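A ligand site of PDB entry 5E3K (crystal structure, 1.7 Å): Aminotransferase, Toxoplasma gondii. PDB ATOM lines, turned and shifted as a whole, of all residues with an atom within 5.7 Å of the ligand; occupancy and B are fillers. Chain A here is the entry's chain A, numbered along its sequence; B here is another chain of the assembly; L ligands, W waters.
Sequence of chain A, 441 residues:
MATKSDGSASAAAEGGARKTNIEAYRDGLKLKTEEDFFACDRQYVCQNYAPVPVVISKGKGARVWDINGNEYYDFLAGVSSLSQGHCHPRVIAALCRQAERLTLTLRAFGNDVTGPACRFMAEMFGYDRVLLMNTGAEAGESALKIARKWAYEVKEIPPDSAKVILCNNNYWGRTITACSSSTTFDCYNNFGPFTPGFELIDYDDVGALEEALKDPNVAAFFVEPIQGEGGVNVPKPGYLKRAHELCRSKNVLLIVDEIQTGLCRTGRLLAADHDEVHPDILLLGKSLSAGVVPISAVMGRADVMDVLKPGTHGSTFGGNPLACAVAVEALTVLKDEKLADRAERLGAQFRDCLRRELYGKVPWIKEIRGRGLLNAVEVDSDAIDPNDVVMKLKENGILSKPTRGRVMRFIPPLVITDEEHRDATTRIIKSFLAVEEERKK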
ATOM      1  N   TYR A  49       3.553   8.121   1.417  1.00  0.00           N
ATOM      2  CA  TYR A  49       4.401   6.985   1.142  1.00  0.00           C
ATOM      3  C   TYR A  49       3.668   5.690   1.508  1.00  0.00           C
ATOM      4  O   TYR A  49       2.976   5.635   2.505  1.00  0.00           O
ATOM      5  CB  TYR A  49       5.666   7.064   1.945  1.00  0.00           C
ATOM      6  CG  TYR A  49       6.706   7.946   1.303  1.00  0.00           C
ATOM      7  CD1 TYR A  49       6.620   9.319   1.401  1.00  0.00           C
ATOM      8  CD2 TYR A  49       7.752   7.399   0.589  1.00  0.00           C
ATOM      9  CE1 TYR A  49       7.542  10.134   0.752  1.00  0.00           C
ATOM     10  CE2 TYR A  49       8.706   8.213  -0.034  1.00  0.00           C
ATOM     11  CZ  TYR A  49       8.583   9.565   0.033  1.00  0.00           C
ATOM     12  OH  TYR A  49       9.537  10.388  -0.591  1.00  0.00           O
ATOM     13  N   GLY A  78      19.386   5.530   0.462  1.00  0.00           N
ATOM     14  CA  GLY A  78      18.857   6.859   0.140  1.00  0.00           C
ATOM     15  C   GLY A  78      18.766   7.115  -1.334  1.00  0.00           C
ATOM     16  O   GLY A  78      18.733   8.262  -1.737  1.00  0.00           O
ATOM     17  N   VAL A  79      18.607   6.044  -2.097  1.00  0.00           N
ATOM     18  CA  VAL A  79      18.733   6.011  -3.574  1.00  0.00           C
ATOM     19  C   VAL A  79      20.006   6.764  -4.002  1.00  0.00           C
ATOM     20  O   VAL A  79      19.960   7.723  -4.812  1.00  0.00           O
ATOM     21  CB  VAL A  79      17.501   6.537  -4.328  1.00  0.00           C
ATOM     22  CG1 VAL A  79      17.529   6.093  -5.803  1.00  0.00           C
ATOM     23  CG2 VAL A  79      16.153   6.057  -3.718  1.00  0.00           C
ATOM     24  N   THR A 135      17.735  20.943  -1.931  1.00  0.00           N
ATOM     25  CA  THR A 135      17.260  19.644  -2.387  1.00  0.00           C
ATOM     26  C   THR A 135      17.514  19.457  -3.912  1.00  0.00           C
ATOM     27  O   THR A 135      17.794  20.406  -4.664  1.00  0.00           O
ATOM     28  CB  THR A 135      15.733  19.474  -2.133  1.00  0.00           C
ATOM     29  OG1 THR A 135      15.043  20.450  -2.937  1.00  0.00           O
ATOM     30  CG2 THR A 135      15.401  19.734  -0.722  1.00  0.00           C
ATOM     31  N   GLY A 136      17.337  18.230  -4.360  1.00  0.00           N
ATOM     32  CA  GLY A 136      17.484  17.938  -5.812  1.00  0.00           C
ATOM     33  C   GLY A 136      16.464  18.685  -6.635  1.00  0.00           C
ATOM     34  O   GLY A 136      16.781  19.265  -7.683  1.00  0.00           O
ATOM     35  N   ALA A 137      15.221  18.734  -6.129  1.00  0.00           N
ATOM     36  CA  ALA A 137      14.182  19.518  -6.829  1.00  0.00           C
ATOM     37  C   ALA A 137      14.608  20.978  -6.986  1.00  0.00           C
ATOM     38  O   ALA A 137      14.398  21.580  -8.042  1.00  0.00           O
ATOM     39  CB  ALA A 137      12.843  19.425  -6.107  1.00  0.00           C
ATOM     40  N   GLU A 138      15.150  21.566  -5.917  1.00  0.00           N
ATOM     41  CA  GLU A 138      15.545  22.932  -6.000  1.00  0.00           C
ATOM     42  C   GLU A 138      16.706  23.146  -7.029  1.00  0.00           C
ATOM     43  O   GLU A 138      16.806  24.194  -7.653  1.00  0.00           O
ATOM     44  CB  GLU A 138      15.982  23.479  -4.644  1.00  0.00           C
ATOM     45  CG  GLU A 138      14.854  23.677  -3.682  1.00  0.00           C
ATOM     46  CD  GLU A 138      15.285  24.432  -2.428  1.00  0.00           C
ATOM     47  OE1 GLU A 138      16.457  24.282  -2.022  1.00  0.00           O
ATOM     48  OE2 GLU A 138      14.466  25.169  -1.862  1.00  0.00           O
ATOM     49  N   TYR A 171      12.665  11.858 -13.794  1.00  0.00           N
ATOM     50  CA  TYR A 171      12.325  12.261 -12.441  1.00  0.00           C
ATOM     51  C   TYR A 171      13.336  13.311 -12.002  1.00  0.00           C
ATOM     52  O   TYR A 171      14.516  13.042 -12.039  1.00  0.00           O
ATOM     53  CB  TYR A 171      12.330  11.103 -11.442  1.00  0.00           C
ATOM     54  CG  TYR A 171      11.816  11.456 -10.069  1.00  0.00           C
ATOM     55  CD1 TYR A 171      12.630  11.999  -9.123  1.00  0.00           C
ATOM     56  CD2 TYR A 171      10.465  11.291  -9.734  1.00  0.00           C
ATOM     57  CE1 TYR A 171      12.146  12.286  -7.873  1.00  0.00           C
ATOM     58  CE2 TYR A 171       9.967  11.645  -8.502  1.00  0.00           C
ATOM     59  CZ  TYR A 171      10.811  12.156  -7.585  1.00  0.00           C
ATOM     60  OH  TYR A 171      10.339  12.464  -6.336  1.00  0.00           O
ATOM     61  N   TRP A 172      12.838  14.439 -11.556  1.00  0.00           N
ATOM     62  CA  TRP A 172      13.701  15.493 -10.964  1.00  0.00           C
ATOM     63  C   TRP A 172      13.104  16.121  -9.727  1.00  0.00           C
ATOM     64  O   TRP A 172      13.678  17.002  -9.149  1.00  0.00           O
ATOM     65  CB  TRP A 172      14.152  16.505 -11.983  1.00  0.00           C
ATOM     66  CG  TRP A 172      13.111  17.426 -12.653  1.00  0.00           C
ATOM     67  CD1 TRP A 172      12.412  17.174 -13.790  1.00  0.00           C
ATOM     68  CD2 TRP A 172      12.739  18.749 -12.240  1.00  0.00           C
ATOM     69  NE1 TRP A 172      11.627  18.227 -14.099  1.00  0.00           N
ATOM     70  CE2 TRP A 172      11.830  19.225 -13.183  1.00  0.00           C
ATOM     71  CE3 TRP A 172      13.060  19.554 -11.159  1.00  0.00           C
ATOM     72  CZ2 TRP A 172      11.253  20.462 -13.080  1.00  0.00           C
ATOM     73  CZ3 TRP A 172      12.470  20.779 -11.056  1.00  0.00           C
ATOM     74  CH2 TRP A 172      11.616  21.248 -12.027  1.00  0.00           C
ATOM     75  N   GLY A 173      11.997  15.604  -9.231  1.00  0.00           N
ATOM     76  CA  GLY A 173      11.430  16.224  -8.068  1.00  0.00           C
ATOM     77  C   GLY A 173       9.942  16.332  -8.085  1.00  0.00           C
ATOM     78  O   GLY A 173       9.285  15.714  -8.927  1.00  0.00           O
ATOM     79  N   ARG A 174       9.451  17.031  -7.067  1.00  0.00           N
ATOM     80  CA  ARG A 174       8.018  17.055  -6.755  1.00  0.00           C
ATOM     81  C   ARG A 174       7.408  18.437  -6.677  1.00  0.00           C
ATOM     82  O   ARG A 174       6.228  18.596  -6.300  1.00  0.00           O
ATOM     83  CB  ARG A 174       7.780  16.281  -5.446  1.00  0.00           C
ATOM     84  CG  ARG A 174       8.177  14.831  -5.521  1.00  0.00           C
ATOM     85  CD  ARG A 174       7.119  14.008  -6.294  1.00  0.00           C
ATOM     86  NE  ARG A 174       7.370  12.604  -6.149  1.00  0.00           N
ATOM     87  CZ  ARG A 174       6.439  11.673  -6.292  1.00  0.00           C
ATOM     88  NH1 ARG A 174       5.215  12.004  -6.666  1.00  0.00           N
ATOM     89  NH2 ARG A 174       6.754  10.428  -6.032  1.00  0.00           N
ATOM     90  N   GLU A 224      18.986  12.735 -17.636  1.00  0.00           N
ATOM     91  CA  GLU A 224      19.709  11.867 -16.691  1.00  0.00           C
ATOM     92  C   GLU A 224      20.679  10.944 -17.456  1.00  0.00           C
ATOM     93  O   GLU A 224      20.285  10.360 -18.434  1.00  0.00           O
ATOM     94  CB  GLU A 224      18.714  11.004 -15.894  1.00  0.00           C
ATOM     95  CG  GLU A 224      17.761  11.789 -14.978  1.00  0.00           C
ATOM     96  CD  GLU A 224      16.596  10.939 -14.479  1.00  0.00           C
ATOM     97  OE1 GLU A 224      16.825  10.165 -13.497  1.00  0.00           O
ATOM     98  OE2 GLU A 224      15.482  11.069 -15.054  1.00  0.00           O
ATOM     99  N   GLY A 228      16.991   7.275 -13.249  1.00  0.00           N
ATOM    100  CA  GLY A 228      17.052   6.731 -11.897  1.00  0.00           C
ATOM    101  C   GLY A 228      15.751   6.109 -11.455  1.00  0.00           C
ATOM    102  O   GLY A 228      15.569   4.878 -11.536  1.00  0.00           O
ATOM    103  N   GLU A 229      14.818   6.941 -11.033  1.00  0.00           N
ATOM    104  CA  GLU A 229      13.466   6.466 -10.654  1.00  0.00           C
ATOM    105  C   GLU A 229      12.756   5.813 -11.808  1.00  0.00           C
ATOM    106  O   GLU A 229      11.870   4.968 -11.568  1.00  0.00           O
ATOM    107  CB  GLU A 229      12.570   7.579 -10.101  1.00  0.00           C
ATOM    108  CG  GLU A 229      13.157   8.312  -8.859  1.00  0.00           C
ATOM    109  CD  GLU A 229      13.478   7.374  -7.698  1.00  0.00           C
ATOM    110  OE1 GLU A 229      12.527   7.020  -6.953  1.00  0.00           O
ATOM    111  OE2 GLU A 229      14.675   6.944  -7.538  1.00  0.00           O
ATOM    112  N   ASP A 257      21.550  15.918 -15.067  1.00  0.00           N
ATOM    113  CA  ASP A 257      21.137  15.651 -13.701  1.00  0.00           C
ATOM    114  C   ASP A 257      21.884  14.461 -13.197  1.00  0.00           C
ATOM    115  O   ASP A 257      21.584  13.331 -13.575  1.00  0.00           O
ATOM    116  CB  ASP A 257      19.632  15.414 -13.628  1.00  0.00           C
ATOM    117  CG  ASP A 257      19.130  15.257 -12.196  1.00  0.00           C
ATOM    118  OD1 ASP A 257      19.958  15.009 -11.289  1.00  0.00           O
ATOM    119  OD2 ASP A 257      17.870  15.342 -11.971  1.00  0.00           O
ATOM    120  N   ILE A 259      22.188  13.971  -9.833  1.00  0.00           N
ATOM    121  CA  ILE A 259      21.752  13.880  -8.431  1.00  0.00           C
ATOM    122  C   ILE A 259      21.794  12.445  -7.921  1.00  0.00           C
ATOM    123  O   ILE A 259      22.253  12.168  -6.821  1.00  0.00           O
ATOM    124  CB  ILE A 259      20.392  14.593  -8.213  1.00  0.00           C
ATOM    125  CG1 ILE A 259      20.607  16.116  -8.378  1.00  0.00           C
ATOM    126  CG2 ILE A 259      19.778  14.328  -6.860  1.00  0.00           C
ATOM    127  CD1 ILE A 259      19.389  16.948  -8.691  1.00  0.00           C
ATOM    128  N   GLN A 260      21.352  11.489  -8.752  1.00  0.00           N
ATOM    129  CA  GLN A 260      21.381  10.078  -8.406  1.00  0.00           C
ATOM    130  C   GLN A 260      22.621   9.315  -8.970  1.00  0.00           C
ATOM    131  O   GLN A 260      23.159   8.415  -8.326  1.00  0.00           O
ATOM    132  CB  GLN A 260      20.057   9.445  -8.851  1.00  0.00           C
ATOM    133  CG  GLN A 260      20.028   7.976  -8.432  1.00  0.00           C
ATOM    134  CD  GLN A 260      18.706   7.275  -8.666  1.00  0.00           C
ATOM    135  OE1 GLN A 260      18.688   6.055  -8.879  1.00  0.00           O
ATOM    136  NE2 GLN A 260      17.599   8.014  -8.628  1.00  0.00           N
ATOM    137  N   LYS A 286      21.977  14.604  -3.131  1.00  0.00           N
ATOM    138  CA  LYS A 286      22.081  13.322  -2.476  1.00  0.00           C
ATOM    139  C   LYS A 286      23.432  13.100  -1.712  1.00  0.00           C
ATOM    140  O   LYS A 286      23.601  13.637  -0.649  1.00  0.00           O
ATOM    141  CB  LYS A 286      21.744  12.231  -3.483  1.00  0.00           C
ATOM    142  CG  LYS A 286      20.226  12.134  -3.734  1.00  0.00           C
ATOM    143  CD  LYS A 286      19.954  10.965  -4.642  1.00  0.00           C
ATOM    144  CE  LYS A 286      18.494  10.780  -5.046  1.00  0.00           C
ATOM    145  NZ  LYS A 286      17.729  10.263  -3.937  1.00  0.00           N
ATOM    146  N   ARG A 409      15.972  -2.861  -7.161  1.00  0.00           N
ATOM    147  CA  ARG A 409      17.178  -1.995  -7.139  1.00  0.00           C
ATOM    148  C   ARG A 409      18.222  -2.447  -6.152  1.00  0.00           C
ATOM    149  O   ARG A 409      17.936  -2.859  -5.030  1.00  0.00           O
ATOM    150  CB  ARG A 409      16.738  -0.574  -6.892  1.00  0.00           C
ATOM    151  CG  ARG A 409      15.815  -0.041  -7.982  1.00  0.00           C
ATOM    152  CD  ARG A 409      15.584   1.452  -7.841  1.00  0.00           C
ATOM    153  NE  ARG A 409      14.755   1.711  -6.676  1.00  0.00           N
ATOM    154  CZ  ARG A 409      14.392   2.914  -6.252  1.00  0.00           C
ATOM    155  NH1 ARG A 409      14.813   4.025  -6.871  1.00  0.00           N
ATOM    156  NH2 ARG A 409      13.535   3.000  -5.253  1.00  0.00           N
ATOM    157  N   LEU B 106      15.204   7.476   4.044  1.00  0.00           N
ATOM    158  CA  LEU B 106      14.087   7.735   3.191  1.00  0.00           C
ATOM    159  C   LEU B 106      12.796   7.313   3.858  1.00  0.00           C
ATOM    160  O   LEU B 106      12.822   6.494   4.790  1.00  0.00           O
ATOM    161  CB  LEU B 106      14.182   6.976   1.863  1.00  0.00           C
ATOM    162  CG  LEU B 106      15.395   7.119   0.980  1.00  0.00           C
ATOM    163  CD1 LEU B 106      15.145   6.153  -0.142  1.00  0.00           C
ATOM    164  CD2 LEU B 106      15.529   8.569   0.484  1.00  0.00           C
ATOM    165  N   ARG B 107      11.680   7.859   3.396  1.00  0.00           N
ATOM    166  CA  ARG B 107      10.391   7.392   3.839  1.00  0.00           C
ATOM    167  C   ARG B 107       9.957   6.059   3.192  1.00  0.00           C
ATOM    168  O   ARG B 107       8.917   5.488   3.546  1.00  0.00           O
ATOM    169  CB  ARG B 107       9.344   8.506   3.682  1.00  0.00           C
ATOM    170  CG  ARG B 107       9.567   9.626   4.706  1.00  0.00           C
ATOM    171  CD  ARG B 107       8.495  10.698   4.694  1.00  0.00           C
ATOM    172  NE  ARG B 107       7.157  10.107   4.911  1.00  0.00           N
ATOM    173  CZ  ARG B 107       6.016  10.663   4.531  1.00  0.00           C
ATOM    174  NH1 ARG B 107       6.000  11.884   4.004  1.00  0.00           N
ATOM    175  NH2 ARG B 107       4.853   9.961   4.678  1.00  0.00           N
ATOM    176  N   ALA B 108      10.759   5.576   2.249  1.00  0.00           N
ATOM    177  CA  ALA B 108      10.687   4.228   1.724  1.00  0.00           C
ATOM    178  C   ALA B 108      10.889   3.130   2.812  1.00  0.00           C
ATOM    179  O   ALA B 108      10.398   1.983   2.679  1.00  0.00           O
ATOM    180  CB  ALA B 108      11.715   4.046   0.617  1.00  0.00           C
ATOM    181  N   GLU B 138       9.539  24.509  -0.582  1.00  0.00           N
ATOM    182  CA  GLU B 138       8.943  23.178  -0.754  1.00  0.00           C
ATOM    183  C   GLU B 138       7.652  23.043   0.045  1.00  0.00           C
ATOM    184  O   GLU B 138       6.760  22.331  -0.354  1.00  0.00           O
ATOM    185  CB  GLU B 138       9.903  22.074  -0.336  1.00  0.00           C
ATOM    186  CG  GLU B 138      11.037  21.845  -1.306  1.00  0.00           C
ATOM    187  CD  GLU B 138      11.888  20.613  -0.963  1.00  0.00           C
ATOM    188  OE1 GLU B 138      12.003  20.196   0.248  1.00  0.00           O
ATOM    189  OE2 GLU B 138      12.413  20.046  -1.952  1.00  0.00           O
ATOM    190  N   GLY B 314       6.632  13.298  -2.628  1.00  0.00           N
ATOM    191  CA  GLY B 314       7.773  12.633  -2.039  1.00  0.00           C
ATOM    192  C   GLY B 314       8.854  13.700  -1.867  1.00  0.00           C
ATOM    193  O   GLY B 314       8.647  14.838  -2.248  1.00  0.00           O
ATOM    194  N   SER B 315       9.944  13.266  -1.323  1.00  0.00           N
ATOM    195  CA  SER B 315      11.183  14.098  -1.097  1.00  0.00           C
ATOM    196  C   SER B 315      12.267  13.140  -0.567  1.00  0.00           C
ATOM    197  O   SER B 315      12.035  12.393   0.393  1.00  0.00           O
ATOM    198  CB  SER B 315      10.913  15.169  -0.038  1.00  0.00           C
ATOM    199  OG  SER B 315      12.148  15.853   0.295  1.00  0.00           O
ATOM    200  N   THR B 316      13.488  13.231  -1.068  1.00  0.00           N
ATOM    201  CA  THR B 316      14.557  12.424  -0.540  1.00  0.00           C
ATOM    202  C   THR B 316      14.780  12.727   0.931  1.00  0.00           C
ATOM    203  O   THR B 316      14.778  11.811   1.794  1.00  0.00           O
ATOM    204  CB  THR B 316      15.896  12.652  -1.310  1.00  0.00           C
ATOM    205  OG1 THR B 316      15.714  12.238  -2.680  1.00  0.00           O
ATOM    206  CG2 THR B 316      17.084  11.903  -0.645  1.00  0.00           C
ATOM    207  N   PHE B 317      15.130  13.965   1.242  1.00  0.00           N
ATOM    208  CA  PHE B 317      15.445  14.288   2.635  1.00  0.00           C
ATOM    209  C   PHE B 317      14.287  14.660   3.561  1.00  0.00           C
ATOM    210  O   PHE B 317      14.492  14.839   4.780  1.00  0.00           O
ATOM    211  CB  PHE B 317      16.523  15.409   2.691  1.00  0.00           C
ATOM    212  CG  PHE B 317      17.893  14.947   2.310  1.00  0.00           C
ATOM    213  CD1 PHE B 317      18.297  14.938   1.011  1.00  0.00           C
ATOM    214  CD2 PHE B 317      18.772  14.501   3.281  1.00  0.00           C
ATOM    215  CE1 PHE B 317      19.571  14.518   0.655  1.00  0.00           C
ATOM    216  CE2 PHE B 317      20.020  14.042   2.955  1.00  0.00           C
ATOM    217  CZ  PHE B 317      20.438  14.060   1.625  1.00  0.00           C
HETATM  218  O1  LIG L   1      11.577   9.195  -1.695  1.00  0.00           O
HETATM  219  C1  LIG L   1      11.890  10.000  -2.617  1.00  0.00           C
HETATM  220  O2  LIG L   1      11.227  10.983  -3.015  1.00  0.00           O
HETATM  221  C2  LIG L   1      13.198   9.714  -3.254  1.00  0.00           C
HETATM  222  C3  LIG L   1      13.382  10.393  -4.600  1.00  0.00           C
HETATM  223  C4  LIG L   1      14.636   9.995  -5.322  1.00  0.00           C
HETATM  224  C5  LIG L   1      15.224   8.856  -5.005  1.00  0.00           C
HETATM  225  N1  LIG L   1      15.264  10.834  -6.409  1.00  0.00           N
HETATM  226  C6  LIG L   1      15.218  12.097  -6.456  1.00  0.00           C
HETATM  227  C7  LIG L   1      15.851  12.839  -7.585  1.00  0.00           C
HETATM  228  C8  LIG L   1      16.539  12.183  -8.627  1.00  0.00           C
HETATM  229  O3  LIG L   1      16.689  10.827  -8.675  1.00  0.00           O
HETATM  230  C9  LIG L   1      17.110  12.932  -9.658  1.00  0.00           C
HETATM  231  C10 LIG L   1      17.864  12.214 -10.761  1.00  0.00           C
HETATM  232  N2  LIG L   1      16.981  14.282  -9.663  1.00  0.00           N
HETATM  233  C11 LIG L   1      16.334  14.929  -8.716  1.00  0.00           C
HETATM  234  C12 LIG L   1      15.731  14.230  -7.660  1.00  0.00           C
HETATM  235  C13 LIG L   1      14.990  15.053  -6.621  1.00  0.00           C
HETATM  236  O4  LIG L   1      15.758  15.189  -5.429  1.00  0.00           O
HETATM  237  P1  LIG L   1      15.061  15.543  -4.030  1.00  0.00           P
HETATM  238  O5  LIG L   1      14.343  14.284  -3.580  1.00  0.00           O
HETATM  239  O6  LIG L   1      16.266  15.906  -3.188  1.00  0.00           O
HETATM  240  O7  LIG L   1      14.171  16.716  -4.262  1.00  0.00           O
HETATM  241  O   HOH W   1      11.456  16.401  -4.712  1.00  0.00           O
HETATM  242  O   HOH W   2      11.752   6.355  -2.115  1.00  0.00           O
HETATM  243  O   HOH W   3      13.079  17.315  -1.761  1.00  0.00           O
HETATM  244  O   HOH W   4      11.690  13.498  -4.345  1.00  0.00           O
HETATM  245  O   HOH W   5      15.409  16.187  -0.568  1.00  0.00           O
HETATM  246  O   HOH W   6      19.232   9.596 -12.574  1.00  0.00           O
HETATM  247  O   HOH W   7      19.342  15.611  -3.224  1.00  0.00           O
HETATM  248  O   HOH W   8       9.373  10.012  -4.707  1.00  0.00           O
HETATM  249  O   HOH W   9      15.637   9.660 -10.918  1.00  0.00           O
HETATM  250  O   HOH W  10      21.042  11.329 -11.708  1.00  0.00           O
HETATM  251  O   HOH W  11      12.156   9.719   1.267  1.00  0.00           O
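Residues that only touch the ligand: Lys 286 (3.1 Å), Val 79 (3.2 Å), Glu 229 (3.2 Å), Tyr 171 (3.4 Å), Trp 172 (3.4 Å), Glu 224 (3.6 Å), Ile 259 (3.7 Å), Thr 135 (3.8 Å) and Gly 314 of chain B (3.8 Å).
Hydrophobic or aromatic side chains within 4 Å of the ligand: Tyr 49, Val 79, Ala 137, Tyr 171 and Ile 259.
The backbone NH of Ser 315 of chain B sits at hydrogen-bond distance from the side-chain hydroxyl of Tyr 49 (3.0 Å).
OG1 of Thr 316 of chain B is in hydrogen-bond range of NZ of Lys 286, 3.1 Å away.
The backbone NH (N) of Ile 259 sits at hydrogen-bond distance from the side-chain carboxylate (OD1) of Asp 257 (2.9 Å).
NE2 of Gln 260 sits at hydrogen-bond distance from OE2 of Glu 229 (3.3 Å).
The backbone carbonyl oxygen of Val 79 lies close to the side-chain amino group of Lys 286 (3.5 Å).
The backbone carbonyl oxygen (O) of Gly 78 lies within hydrogen-bond range of the side-chain amino group (NZ) of Lys 286 (3.1 Å).
The guanidinium group (NH1) of Arg 409 is in salt-bridge range of the side-chain carboxylate (OE2) of Glu 229.
NE of Arg 174 sits at hydrogen-bond distance from OH of Tyr 171, at 3.0 Å.
An oxygen (O1) of the ligand is in hydrogen-bond range of the side-chain hydroxyl (OH) of Tyr 49 (2.6 Å).
O5 of the ligand lies within hydrogen-bond range of N of Thr 316 of chain B, 2.9 Å away.
OG1 of Thr 316 of chain B lies within hydrogen-bond range of O5 of the ligand (2.6 Å).
The side-chain carboxylate of Asp 257 sits at hydrogen-bond distance from a nitrogen (N2) of the ligand (2.7 Å).
O6 of the ligand lies within hydrogen-bond range of N of Gly 136, at 2.8 Å.
The backbone NH (N) of Ala 137 is in hydrogen-bond range of an oxygen (O7) of the ligand (2.9 Å).
An oxygen (O3) of the ligand lies within hydrogen-bond range of the side-chain amide nitrogen (NE2) of Gln 260, at 3.0 Å.
N of Ser 315 of chain B lies within hydrogen-bond range of O2 of the ligand, at 3.1 Å.
Water W8 lies within hydrogen-bond range of an oxygen (O2) of the ligand (2.7 Å), the guanidinium group (NH2) of Arg 174 (3.0 Å) and the side-chain hydroxyl (OH) of Tyr 171 (3.1 Å).
Water W9 lies within hydrogen-bond range of O3 of the ligand (2.7 Å), N of Glu 229 (2.8 Å), OE1 of Glu 224 (2.9 Å) and NE2 of Gln 260 (3.4 Å).
Water W1 lies within hydrogen-bond range of O7 of the ligand (2.8 Å) and N of Arg 174 (3.2 Å).
Water W5 lies within hydrogen-bond range of O6 of the ligand, N of Phe 317 of chain B and OG of Ser 315 of chain B.
Water W3 lies within hydrogen-bond range of the side-chain hydroxyl (OG) of Ser 315 of chain B (2.7 Å), an oxygen (O7) of the ligand (2.8 Å) and the side-chain carboxylate (OE2) of Glu 138 of chain B (2.8 Å).
Water W6 bridges OE1 of Glu 224 (2.6 Å) and N of Gly 228 (3.3 Å).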
